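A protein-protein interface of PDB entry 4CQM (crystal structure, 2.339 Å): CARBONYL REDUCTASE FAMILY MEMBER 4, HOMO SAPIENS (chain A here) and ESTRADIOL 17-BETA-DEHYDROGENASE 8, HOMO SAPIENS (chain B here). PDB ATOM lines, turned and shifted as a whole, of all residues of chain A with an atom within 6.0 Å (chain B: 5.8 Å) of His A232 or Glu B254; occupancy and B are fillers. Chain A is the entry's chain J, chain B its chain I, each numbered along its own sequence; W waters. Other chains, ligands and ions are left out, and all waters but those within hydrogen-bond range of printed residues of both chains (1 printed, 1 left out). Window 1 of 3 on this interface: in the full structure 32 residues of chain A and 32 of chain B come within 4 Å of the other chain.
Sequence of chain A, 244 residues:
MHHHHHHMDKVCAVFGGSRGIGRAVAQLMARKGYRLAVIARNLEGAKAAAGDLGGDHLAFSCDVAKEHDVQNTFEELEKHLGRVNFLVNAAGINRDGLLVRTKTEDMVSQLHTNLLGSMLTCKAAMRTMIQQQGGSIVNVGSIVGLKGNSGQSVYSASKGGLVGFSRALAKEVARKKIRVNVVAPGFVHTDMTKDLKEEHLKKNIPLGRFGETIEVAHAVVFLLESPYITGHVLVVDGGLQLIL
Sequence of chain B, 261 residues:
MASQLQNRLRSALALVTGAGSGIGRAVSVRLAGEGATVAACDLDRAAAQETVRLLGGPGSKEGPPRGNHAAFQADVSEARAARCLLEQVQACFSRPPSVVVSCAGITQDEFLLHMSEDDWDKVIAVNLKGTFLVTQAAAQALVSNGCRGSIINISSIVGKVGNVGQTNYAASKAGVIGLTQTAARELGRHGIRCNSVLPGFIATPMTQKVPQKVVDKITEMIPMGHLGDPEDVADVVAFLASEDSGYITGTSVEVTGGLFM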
ATOM      1  N   ARG A 167     -20.641  13.358 -27.357  1.00  0.00           N
ATOM      2  CA  ARG A 167     -21.216  12.021 -27.276  1.00  0.00           C
ATOM      3  C   ARG A 167     -22.721  12.050 -27.520  1.00  0.00           C
ATOM      4  O   ARG A 167     -23.268  11.169 -28.184  1.00  0.00           O
ATOM      5  CB  ARG A 167     -20.908  11.388 -25.920  1.00  0.00           C
ATOM      6  CG  ARG A 167     -19.476  10.897 -25.790  1.00  0.00           C
ATOM      7  CD  ARG A 167     -19.214  10.284 -24.426  1.00  0.00           C
ATOM      8  NE  ARG A 167     -17.883   9.691 -24.341  1.00  0.00           N
ATOM      9  CZ  ARG A 167     -17.341   9.228 -23.221  1.00  0.00           C
ATOM     10  NH1 ARG A 167     -18.014   9.294 -22.080  1.00  0.00           N
ATOM     11  NH2 ARG A 167     -16.123   8.704 -23.239  1.00  0.00           N
ATOM     12  N   VAL A 180     -18.702  11.984 -34.446  1.00  0.00           N
ATOM     13  CA  VAL A 180     -18.209  13.031 -33.558  1.00  0.00           C
ATOM     14  C   VAL A 180     -17.302  12.429 -32.490  1.00  0.00           C
ATOM     15  O   VAL A 180     -17.694  11.500 -31.784  1.00  0.00           O
ATOM     16  CB  VAL A 180     -19.362  13.795 -32.879  1.00  0.00           C
ATOM     17  CG1 VAL A 180     -18.829  15.019 -32.152  1.00  0.00           C
ATOM     18  CG2 VAL A 180     -20.412  14.199 -33.903  1.00  0.00           C
ATOM     19  N   ASN A 181     -16.087  12.957 -32.377  1.00  0.00           N
ATOM     20  CA  ASN A 181     -15.111  12.435 -31.428  1.00  0.00           C
ATOM     21  C   ASN A 181     -14.358  13.535 -30.691  1.00  0.00           C
ATOM     22  O   ASN A 181     -14.387  14.697 -31.093  1.00  0.00           O
ATOM     23  CB  ASN A 181     -14.116  11.520 -32.143  1.00  0.00           C
ATOM     24  CG  ASN A 181     -14.695  10.157 -32.450  1.00  0.00           C
ATOM     25  OD1 ASN A 181     -15.293   9.518 -31.585  1.00  0.00           O
ATOM     26  ND2 ASN A 181     -14.528   9.708 -33.687  1.00  0.00           N
ATOM     27  N   VAL A 182     -13.684  13.156 -29.610  1.00  0.00           N
ATOM     28  CA  VAL A 182     -12.924  14.107 -28.807  1.00  0.00           C
ATOM     29  C   VAL A 182     -11.473  13.671 -28.645  1.00  0.00           C
ATOM     30  O   VAL A 182     -11.195  12.531 -28.273  1.00  0.00           O
ATOM     31  CB  VAL A 182     -13.548  14.290 -27.404  1.00  0.00           C
ATOM     32  CG1 VAL A 182     -12.655  15.156 -26.524  1.00  0.00           C
ATOM     33  CG2 VAL A 182     -14.934  14.894 -27.512  1.00  0.00           C
ATOM     34  N   VAL A 183     -10.551  14.581 -28.936  1.00  0.00           N
ATOM     35  CA  VAL A 183      -9.143  14.360 -28.635  1.00  0.00           C
ATOM     36  C   VAL A 183      -8.832  14.942 -27.264  1.00  0.00           C
ATOM     37  O   VAL A 183      -9.163  16.093 -26.983  1.00  0.00           O
ATOM     38  CB  VAL A 183      -8.219  14.992 -29.695  1.00  0.00           C
ATOM     39  CG1 VAL A 183      -6.778  15.019 -29.206  1.00  0.00           C
ATOM     40  CG2 VAL A 183      -8.323  14.235 -31.007  1.00  0.00           C
ATOM     41  N   LEU A 223      -8.784  10.028 -35.815  1.00  0.00           N
ATOM     42  CA  LEU A 223     -10.202   9.969 -35.480  1.00  0.00           C
ATOM     43  C   LEU A 223     -11.071  10.377 -36.664  1.00  0.00           C
ATOM     44  O   LEU A 223     -12.157   9.835 -36.864  1.00  0.00           O
ATOM     45  CB  LEU A 223     -10.509  10.861 -34.276  1.00  0.00           C
ATOM     46  CG  LEU A 223     -10.057  10.333 -32.914  1.00  0.00           C
ATOM     47  CD1 LEU A 223     -10.383  11.335 -31.821  1.00  0.00           C
ATOM     48  CD2 LEU A 223     -10.705   8.988 -32.622  1.00  0.00           C
ATOM     49  N   TYR A 228     -15.205   3.548 -37.929  1.00  0.00           N
ATOM     50  CA  TYR A 228     -16.047   2.884 -36.937  1.00  0.00           C
ATOM     51  C   TYR A 228     -15.769   3.406 -35.531  1.00  0.00           C
ATOM     52  O   TYR A 228     -15.850   2.664 -34.554  1.00  0.00           O
ATOM     53  CB  TYR A 228     -15.844   1.369 -36.991  1.00  0.00           C
ATOM     54  CG  TYR A 228     -16.996   0.569 -36.421  1.00  0.00           C
ATOM     55  CD1 TYR A 228     -18.256   0.617 -37.005  1.00  0.00           C
ATOM     56  CD2 TYR A 228     -16.822  -0.246 -35.309  1.00  0.00           C
ATOM     57  CE1 TYR A 228     -19.311  -0.114 -36.492  1.00  0.00           C
ATOM     58  CE2 TYR A 228     -17.870  -0.981 -34.790  1.00  0.00           C
ATOM     59  CZ  TYR A 228     -19.113  -0.912 -35.384  1.00  0.00           C
ATOM     60  OH  TYR A 228     -20.158  -1.643 -34.869  1.00  0.00           O
ATOM     61  N   ILE A 229     -15.442   4.690 -35.436  1.00  0.00           N
ATOM     62  CA  ILE A 229     -15.189   5.321 -34.146  1.00  0.00           C
ATOM     63  C   ILE A 229     -15.971   6.622 -34.009  1.00  0.00           C
ATOM     64  O   ILE A 229     -15.695   7.601 -34.704  1.00  0.00           O
ATOM     65  CB  ILE A 229     -13.685   5.610 -33.936  1.00  0.00           C
ATOM     66  CG1 ILE A 229     -12.886   4.305 -33.911  1.00  0.00           C
ATOM     67  CG2 ILE A 229     -13.467   6.388 -32.648  1.00  0.00           C
ATOM     68  CD1 ILE A 229     -11.414   4.490 -33.600  1.00  0.00           C
ATOM     69  N   THR A 230     -16.957   6.624 -33.117  1.00  0.00           N
ATOM     70  CA  THR A 230     -17.710   7.835 -32.818  1.00  0.00           C
ATOM     71  C   THR A 230     -18.008   7.920 -31.325  1.00  0.00           C
ATOM     72  O   THR A 230     -18.102   6.899 -30.639  1.00  0.00           O
ATOM     73  CB  THR A 230     -19.030   7.906 -33.614  1.00  0.00           C
ATOM     74  OG1 THR A 230     -19.636   9.192 -33.425  1.00  0.00           O
ATOM     75  CG2 THR A 230     -19.999   6.826 -33.161  1.00  0.00           C
ATOM     76  N   GLY A 231     -18.145   9.145 -30.826  1.00  0.00           N
ATOM     77  CA  GLY A 231     -18.418   9.373 -29.418  1.00  0.00           C
ATOM     78  C   GLY A 231     -17.287   8.906 -28.522  1.00  0.00           C
ATOM     79  O   GLY A 231     -17.507   8.555 -27.364  1.00  0.00           O
ATOM     80  N   HIS A 232     -16.072   8.905 -29.059  1.00  0.00           N
ATOM     81  CA  HIS A 232     -14.915   8.427 -28.315  1.00  0.00           C
ATOM     82  C   HIS A 232     -13.990   9.563 -27.894  1.00  0.00           C
ATOM     83  O   HIS A 232     -13.841  10.558 -28.604  1.00  0.00           O
ATOM     84  CB  HIS A 232     -14.132   7.406 -29.142  1.00  0.00           C
ATOM     85  CG  HIS A 232     -12.851   6.972 -28.504  1.00  0.00           C
ATOM     86  ND1 HIS A 232     -11.614   7.327 -28.998  1.00  0.00           N
ATOM     87  CD2 HIS A 232     -12.614   6.227 -27.398  1.00  0.00           C
ATOM     88  CE1 HIS A 232     -10.671   6.809 -28.232  1.00  0.00           C
ATOM     89  NE2 HIS A 232     -11.250   6.137 -27.253  1.00  0.00           N
ATOM     90  N   VAL A 233     -13.374   9.404 -26.727  1.00  0.00           N
ATOM     91  CA  VAL A 233     -12.398  10.364 -26.234  1.00  0.00           C
ATOM     92  C   VAL A 233     -10.995   9.771 -26.313  1.00  0.00           C
ATOM     93  O   VAL A 233     -10.606   8.954 -25.477  1.00  0.00           O
ATOM     94  CB  VAL A 233     -12.696  10.784 -24.784  1.00  0.00           C
ATOM     95  CG1 VAL A 233     -11.703  11.840 -24.322  1.00  0.00           C
ATOM     96  CG2 VAL A 233     -14.121  11.300 -24.667  1.00  0.00           C
ATOM     97  N   LEU A 234     -10.241  10.179 -27.329  1.00  0.00           N
ATOM     98  CA  LEU A 234      -8.878   9.693 -27.507  1.00  0.00           C
ATOM     99  C   LEU A 234      -7.907  10.480 -26.636  1.00  0.00           C
ATOM    100  O   LEU A 234      -7.843  11.707 -26.714  1.00  0.00           O
ATOM    101  CB  LEU A 234      -8.464   9.778 -28.977  1.00  0.00           C
ATOM    102  CG  LEU A 234      -7.075   9.237 -29.318  1.00  0.00           C
ATOM    103  CD1 LEU A 234      -6.934   7.795 -28.861  1.00  0.00           C
ATOM    104  CD2 LEU A 234      -6.810   9.356 -30.811  1.00  0.00           C
ATOM    105  N   VAL A 235      -7.151   9.767 -25.809  1.00  0.00           N
ATOM    106  CA  VAL A 235      -6.242  10.405 -24.866  1.00  0.00           C
ATOM    107  C   VAL A 235      -4.801  10.406 -25.369  1.00  0.00           C
ATOM    108  O   VAL A 235      -4.217   9.350 -25.613  1.00  0.00           O
ATOM    109  CB  VAL A 235      -6.291   9.710 -23.494  1.00  0.00           C
ATOM    110  CG1 VAL A 235      -5.357  10.400 -22.520  1.00  0.00           C
ATOM    111  CG2 VAL A 235      -7.714   9.699 -22.958  1.00  0.00           C
ATOM    112  N   ILE B 157     -15.108  -3.746 -25.650  1.00  0.00           N
ATOM    113  CA  ILE B 157     -16.016  -2.781 -25.043  1.00  0.00           C
ATOM    114  C   ILE B 157     -16.732  -3.450 -23.869  1.00  0.00           C
ATOM    115  O   ILE B 157     -17.224  -2.782 -22.958  1.00  0.00           O
ATOM    116  CB  ILE B 157     -17.039  -2.233 -26.066  1.00  0.00           C
ATOM    117  CG1 ILE B 157     -17.778  -1.020 -25.495  1.00  0.00           C
ATOM    118  CG2 ILE B 157     -18.012  -3.320 -26.506  1.00  0.00           C
ATOM    119  CD1 ILE B 157     -16.865   0.129 -25.123  1.00  0.00           C
ATOM    120  N   LYS B 160     -15.370  -2.846 -20.382  1.00  0.00           N
ATOM    121  CA  LYS B 160     -15.643  -1.560 -19.753  1.00  0.00           C
ATOM    122  C   LYS B 160     -17.031  -1.527 -19.113  1.00  0.00           C
ATOM    123  O   LYS B 160     -17.242  -0.841 -18.114  1.00  0.00           O
ATOM    124  CB  LYS B 160     -15.514  -0.425 -20.772  1.00  0.00           C
ATOM    125  CG  LYS B 160     -15.505   0.963 -20.149  1.00  0.00           C
ATOM    126  CD  LYS B 160     -15.562   2.061 -21.200  1.00  0.00           C
ATOM    127  CE  LYS B 160     -16.914   2.094 -21.896  1.00  0.00           C
ATOM    128  NZ  LYS B 160     -17.026   3.238 -22.844  1.00  0.00           N
ATOM    129  N   SER B 196      -4.580  -0.347 -25.245  1.00  0.00           N
ATOM    130  CA  SER B 196      -5.624  -1.349 -25.406  1.00  0.00           C
ATOM    131  C   SER B 196      -6.669  -0.911 -26.421  1.00  0.00           C
ATOM    132  O   SER B 196      -7.089   0.245 -26.438  1.00  0.00           O
ATOM    133  CB  SER B 196      -6.296  -1.647 -24.064  1.00  0.00           C
ATOM    134  OG  SER B 196      -5.431  -2.375 -23.212  1.00  0.00           O
ATOM    135  N   VAL B 197      -7.080  -1.845 -27.271  1.00  0.00           N
ATOM    136  CA  VAL B 197      -8.154  -1.595 -28.220  1.00  0.00           C
ATOM    137  C   VAL B 197      -9.452  -2.173 -27.669  1.00  0.00           C
ATOM    138  O   VAL B 197      -9.482  -3.313 -27.207  1.00  0.00           O
ATOM    139  CB  VAL B 197      -7.851  -2.208 -29.601  1.00  0.00           C
ATOM    140  CG1 VAL B 197      -9.002  -1.957 -30.563  1.00  0.00           C
ATOM    141  CG2 VAL B 197      -6.555  -1.640 -30.157  1.00  0.00           C
ATOM    142  N   LEU B 198     -10.516  -1.377 -27.705  1.00  0.00           N
ATOM    143  CA  LEU B 198     -11.812  -1.803 -27.186  1.00  0.00           C
ATOM    144  C   LEU B 198     -12.858  -1.857 -28.294  1.00  0.00           C
ATOM    145  O   LEU B 198     -13.638  -0.920 -28.461  1.00  0.00           O
ATOM    146  CB  LEU B 198     -12.283  -0.865 -26.071  1.00  0.00           C
ATOM    147  CG  LEU B 198     -11.756  -1.079 -24.649  1.00  0.00           C
ATOM    148  CD1 LEU B 198     -10.254  -0.847 -24.554  1.00  0.00           C
ATOM    149  CD2 LEU B 198     -12.500  -0.178 -23.675  1.00  0.00           C
ATOM    150  N   PRO B 199     -12.877  -2.958 -29.057  1.00  0.00           N
ATOM    151  CA  PRO B 199     -13.814  -3.091 -30.174  1.00  0.00           C
ATOM    152  C   PRO B 199     -15.225  -3.446 -29.720  1.00  0.00           C
ATOM    153  O   PRO B 199     -15.392  -4.146 -28.721  1.00  0.00           O
ATOM    154  CB  PRO B 199     -13.215  -4.235 -31.009  1.00  0.00           C
ATOM    155  CG  PRO B 199     -11.846  -4.499 -30.422  1.00  0.00           C
ATOM    156  CD  PRO B 199     -11.951  -4.099 -28.992  1.00  0.00           C
ATOM    157  N   SER B 252      -6.952   3.568 -23.768  1.00  0.00           N
ATOM    158  CA  SER B 252      -7.957   2.651 -24.288  1.00  0.00           C
ATOM    159  C   SER B 252      -8.706   3.292 -25.453  1.00  0.00           C
ATOM    160  O   SER B 252      -9.422   4.277 -25.274  1.00  0.00           O
ATOM    161  CB  SER B 252      -8.936   2.247 -23.185  1.00  0.00           C
ATOM    162  OG  SER B 252      -8.253   1.677 -22.083  1.00  0.00           O
ATOM    163  N   VAL B 253      -8.534   2.735 -26.647  1.00  0.00           N
ATOM    164  CA  VAL B 253      -9.191   3.270 -27.833  1.00  0.00           C
ATOM    165  C   VAL B 253     -10.440   2.464 -28.177  1.00  0.00           C
ATOM    166  O   VAL B 253     -10.367   1.255 -28.399  1.00  0.00           O
ATOM    167  CB  VAL B 253      -8.245   3.280 -29.047  1.00  0.00           C
ATOM    168  CG1 VAL B 253      -8.932   3.915 -30.246  1.00  0.00           C
ATOM    169  CG2 VAL B 253      -6.961   4.023 -28.708  1.00  0.00           C
ATOM    170  N   GLU B 254     -11.583   3.140 -28.218  1.00  0.00           N
ATOM    171  CA  GLU B 254     -12.851   2.476 -28.499  1.00  0.00           C
ATOM    172  C   GLU B 254     -13.208   2.527 -29.979  1.00  0.00           C
ATOM    173  O   GLU B 254     -13.290   3.600 -30.575  1.00  0.00           O
ATOM    174  CB  GLU B 254     -13.982   3.107 -27.681  1.00  0.00           C
ATOM    175  CG  GLU B 254     -13.795   3.025 -26.176  1.00  0.00           C
ATOM    176  CD  GLU B 254     -14.985   3.578 -25.414  1.00  0.00           C
ATOM    177  OE1 GLU B 254     -16.026   3.851 -26.049  1.00  0.00           O
ATOM    178  OE2 GLU B 254     -14.881   3.741 -24.180  1.00  0.00           O
ATOM    179  N   VAL B 255     -13.416   1.355 -30.567  1.00  0.00           N
ATOM    180  CA  VAL B 255     -13.931   1.258 -31.925  1.00  0.00           C
ATOM    181  C   VAL B 255     -15.212   0.419 -31.866  1.00  0.00           C
ATOM    182  O   VAL B 255     -15.209  -0.794 -32.084  1.00  0.00           O
ATOM    183  CB  VAL B 255     -12.870   0.669 -32.902  1.00  0.00           C
ATOM    184  CG1 VAL B 255     -12.192  -0.573 -32.316  1.00  0.00           C
ATOM    185  CG2 VAL B 255     -13.464   0.402 -34.284  1.00  0.00           C
ATOM    186  N   THR B 256     -16.313   1.087 -31.536  1.00  0.00           N
ATOM    187  CA  THR B 256     -17.560   0.400 -31.221  1.00  0.00           C
ATOM    188  C   THR B 256     -18.726   0.851 -32.092  1.00  0.00           C
ATOM    189  O   THR B 256     -19.793   0.238 -32.079  1.00  0.00           O
ATOM    190  CB  THR B 256     -17.948   0.616 -29.748  1.00  0.00           C
ATOM    191  OG1 THR B 256     -18.243   2.002 -29.531  1.00  0.00           O
ATOM    192  CG2 THR B 256     -16.811   0.196 -28.831  1.00  0.00           C
ATOM    193  N   LEU B 259     -21.339   2.266 -29.665  1.00  0.00           N
ATOM    194  CA  LEU B 259     -21.989   1.344 -28.743  1.00  0.00           C
ATOM    195  C   LEU B 259     -21.380   1.440 -27.348  1.00  0.00           C
ATOM    196  O   LEU B 259     -20.167   1.303 -27.183  1.00  0.00           O
ATOM    197  CB  LEU B 259     -21.891  -0.092 -29.263  1.00  0.00           C
ATOM    198  CG  LEU B 259     -22.723  -1.142 -28.520  1.00  0.00           C
ATOM    199  CD1 LEU B 259     -24.207  -0.829 -28.633  1.00  0.00           C
ATOM    200  CD2 LEU B 259     -22.426  -2.537 -29.049  1.00  0.00           C
ATOM    201  N   PHE B 260     -22.236   1.687 -26.358  1.00  0.00           N
ATOM    202  CA  PHE B 260     -21.836   1.765 -24.952  1.00  0.00           C
ATOM    203  C   PHE B 260     -20.768   2.830 -24.712  1.00  0.00           C
ATOM    204  O   PHE B 260     -19.885   2.656 -23.870  1.00  0.00           O
ATOM    205  CB  PHE B 260     -21.334   0.405 -24.458  1.00  0.00           C
ATOM    206  CG  PHE B 260     -22.340  -0.704 -24.597  1.00  0.00           C
ATOM    207  CD1 PHE B 260     -23.701  -0.436 -24.580  1.00  0.00           C
ATOM    208  CD2 PHE B 260     -21.924  -2.018 -24.744  1.00  0.00           C
ATOM    209  CE1 PHE B 260     -24.625  -1.457 -24.708  1.00  0.00           C
ATOM    210  CE2 PHE B 260     -22.843  -3.042 -24.871  1.00  0.00           C
ATOM    211  CZ  PHE B 260     -24.195  -2.761 -24.853  1.00  0.00           C
ATOM    212  N   MET B 261     -20.853   3.930 -25.455  1.00  0.00           N
ATOM    213  CA  MET B 261     -19.889   5.018 -25.333  1.00  0.00           C
ATOM    214  C   MET B 261     -19.984   5.698 -23.971  1.00  0.00           C
ATOM    215  O   MET B 261     -18.983   5.852 -23.270  1.00  0.00           O
ATOM    216  CB  MET B 261     -20.102   6.051 -26.441  1.00  0.00           C
ATOM    217  CG  MET B 261     -21.426   6.790 -26.337  1.00  0.00           C
ATOM    218  SD  MET B 261     -21.538   8.243 -27.400  1.00  0.00           S
ATOM    219  CE  MET B 261     -21.605   7.494 -29.023  1.00  0.00           C
HETATM  220  O   HOH W   1     -16.031   3.996 -31.069  1.00  0.00           O
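The backbone carbonyl oxygen of Arg A167 sits close to the side-chain sulfur of Met B261.
A ring nitrogen (NE2) of His A232 is in hydrogen-bond range of the backbone NH (N) of Glu B254 (3.2 Å).
OH of Tyr A228 sits at hydrogen-bond distance from O of Thr B256.
The backbone carbonyl oxygen (O) of Ser B252 sits at hydrogen-bond distance from a ring nitrogen (NE2) of His A232, at 3.3 Å.
N of His A232 is in hydrogen-bond range of OD1 of Asn A181 (2.7 Å).
The backbone NH (N) of Val B255 sits at hydrogen-bond distance from the backbone carbonyl oxygen (O) of Leu B198 (3.1 Å).
The side-chain amide oxygen of Asn A181 lies within hydrogen-bond range of the backbone NH of Gly A231, 3.0 Å away.
The backbone carbonyl oxygen (O) of Val B253 is in hydrogen-bond range of the backbone NH (N) of Leu B198, 2.7 Å away.
O of Val A180 lies within hydrogen-bond range of N of Gly A231, at 2.6 Å.
NZ of Lys B160 is in salt-bridge range of OE2 of Glu B254 (2.6 Å).
Tyr A228 touches Val B255 (O to CG2, 3.3 Å).
Ile A229 touches Glu B254 (CG1 to O, 3.4 Å).
CG1 of Ile A229 touches CB of Val B255, 3.8 Å away.
Thr A230 touches Met B261.
CA of Gly A231 touches CE of Met B261, 3.7 Å away.
Val B253 touches His A232.
Val B253 touches Leu A234 (CG2 to CD1, 3.8 Å).
Val A182 touches none of the printed residues of chain B.
His A232 touches three residues of chain B.
Of the printed residues of chain B, Leu A234 touches Val B253 (3.8 Å).
Val A235 touches none of the printed residues of chain B.
Glu B254 touches just these residues of chain A: Ile A229 and His A232.
Printed residues of chain A within 4 Å of Thr B256: Tyr A228.
Of the printed residues of chain A, Met B261 touches Arg A167 (3.5 Å), Thr A230 (3.9 Å) and Gly A231 (3.7 Å).
Of the 14 printed residues of chain B, 6 touch a printed residue of chain A.
Hydrophobic or aromatic side chains of chain B that line the printed part of chain A: Val B253, Val B255 and Met B261.
Hydrophobic or aromatic side chains of chain A that line the printed part of chain B: Tyr A228, Ile A229, His A232 and Leu A234.
Among the printed residues, 11 pairs touch across the chains.
Water W1 lies within hydrogen-bond range of O of Glu B254 (2.8 Å), N of Thr B256 (3.0 Å) and N of Thr A230 (3.5 Å).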
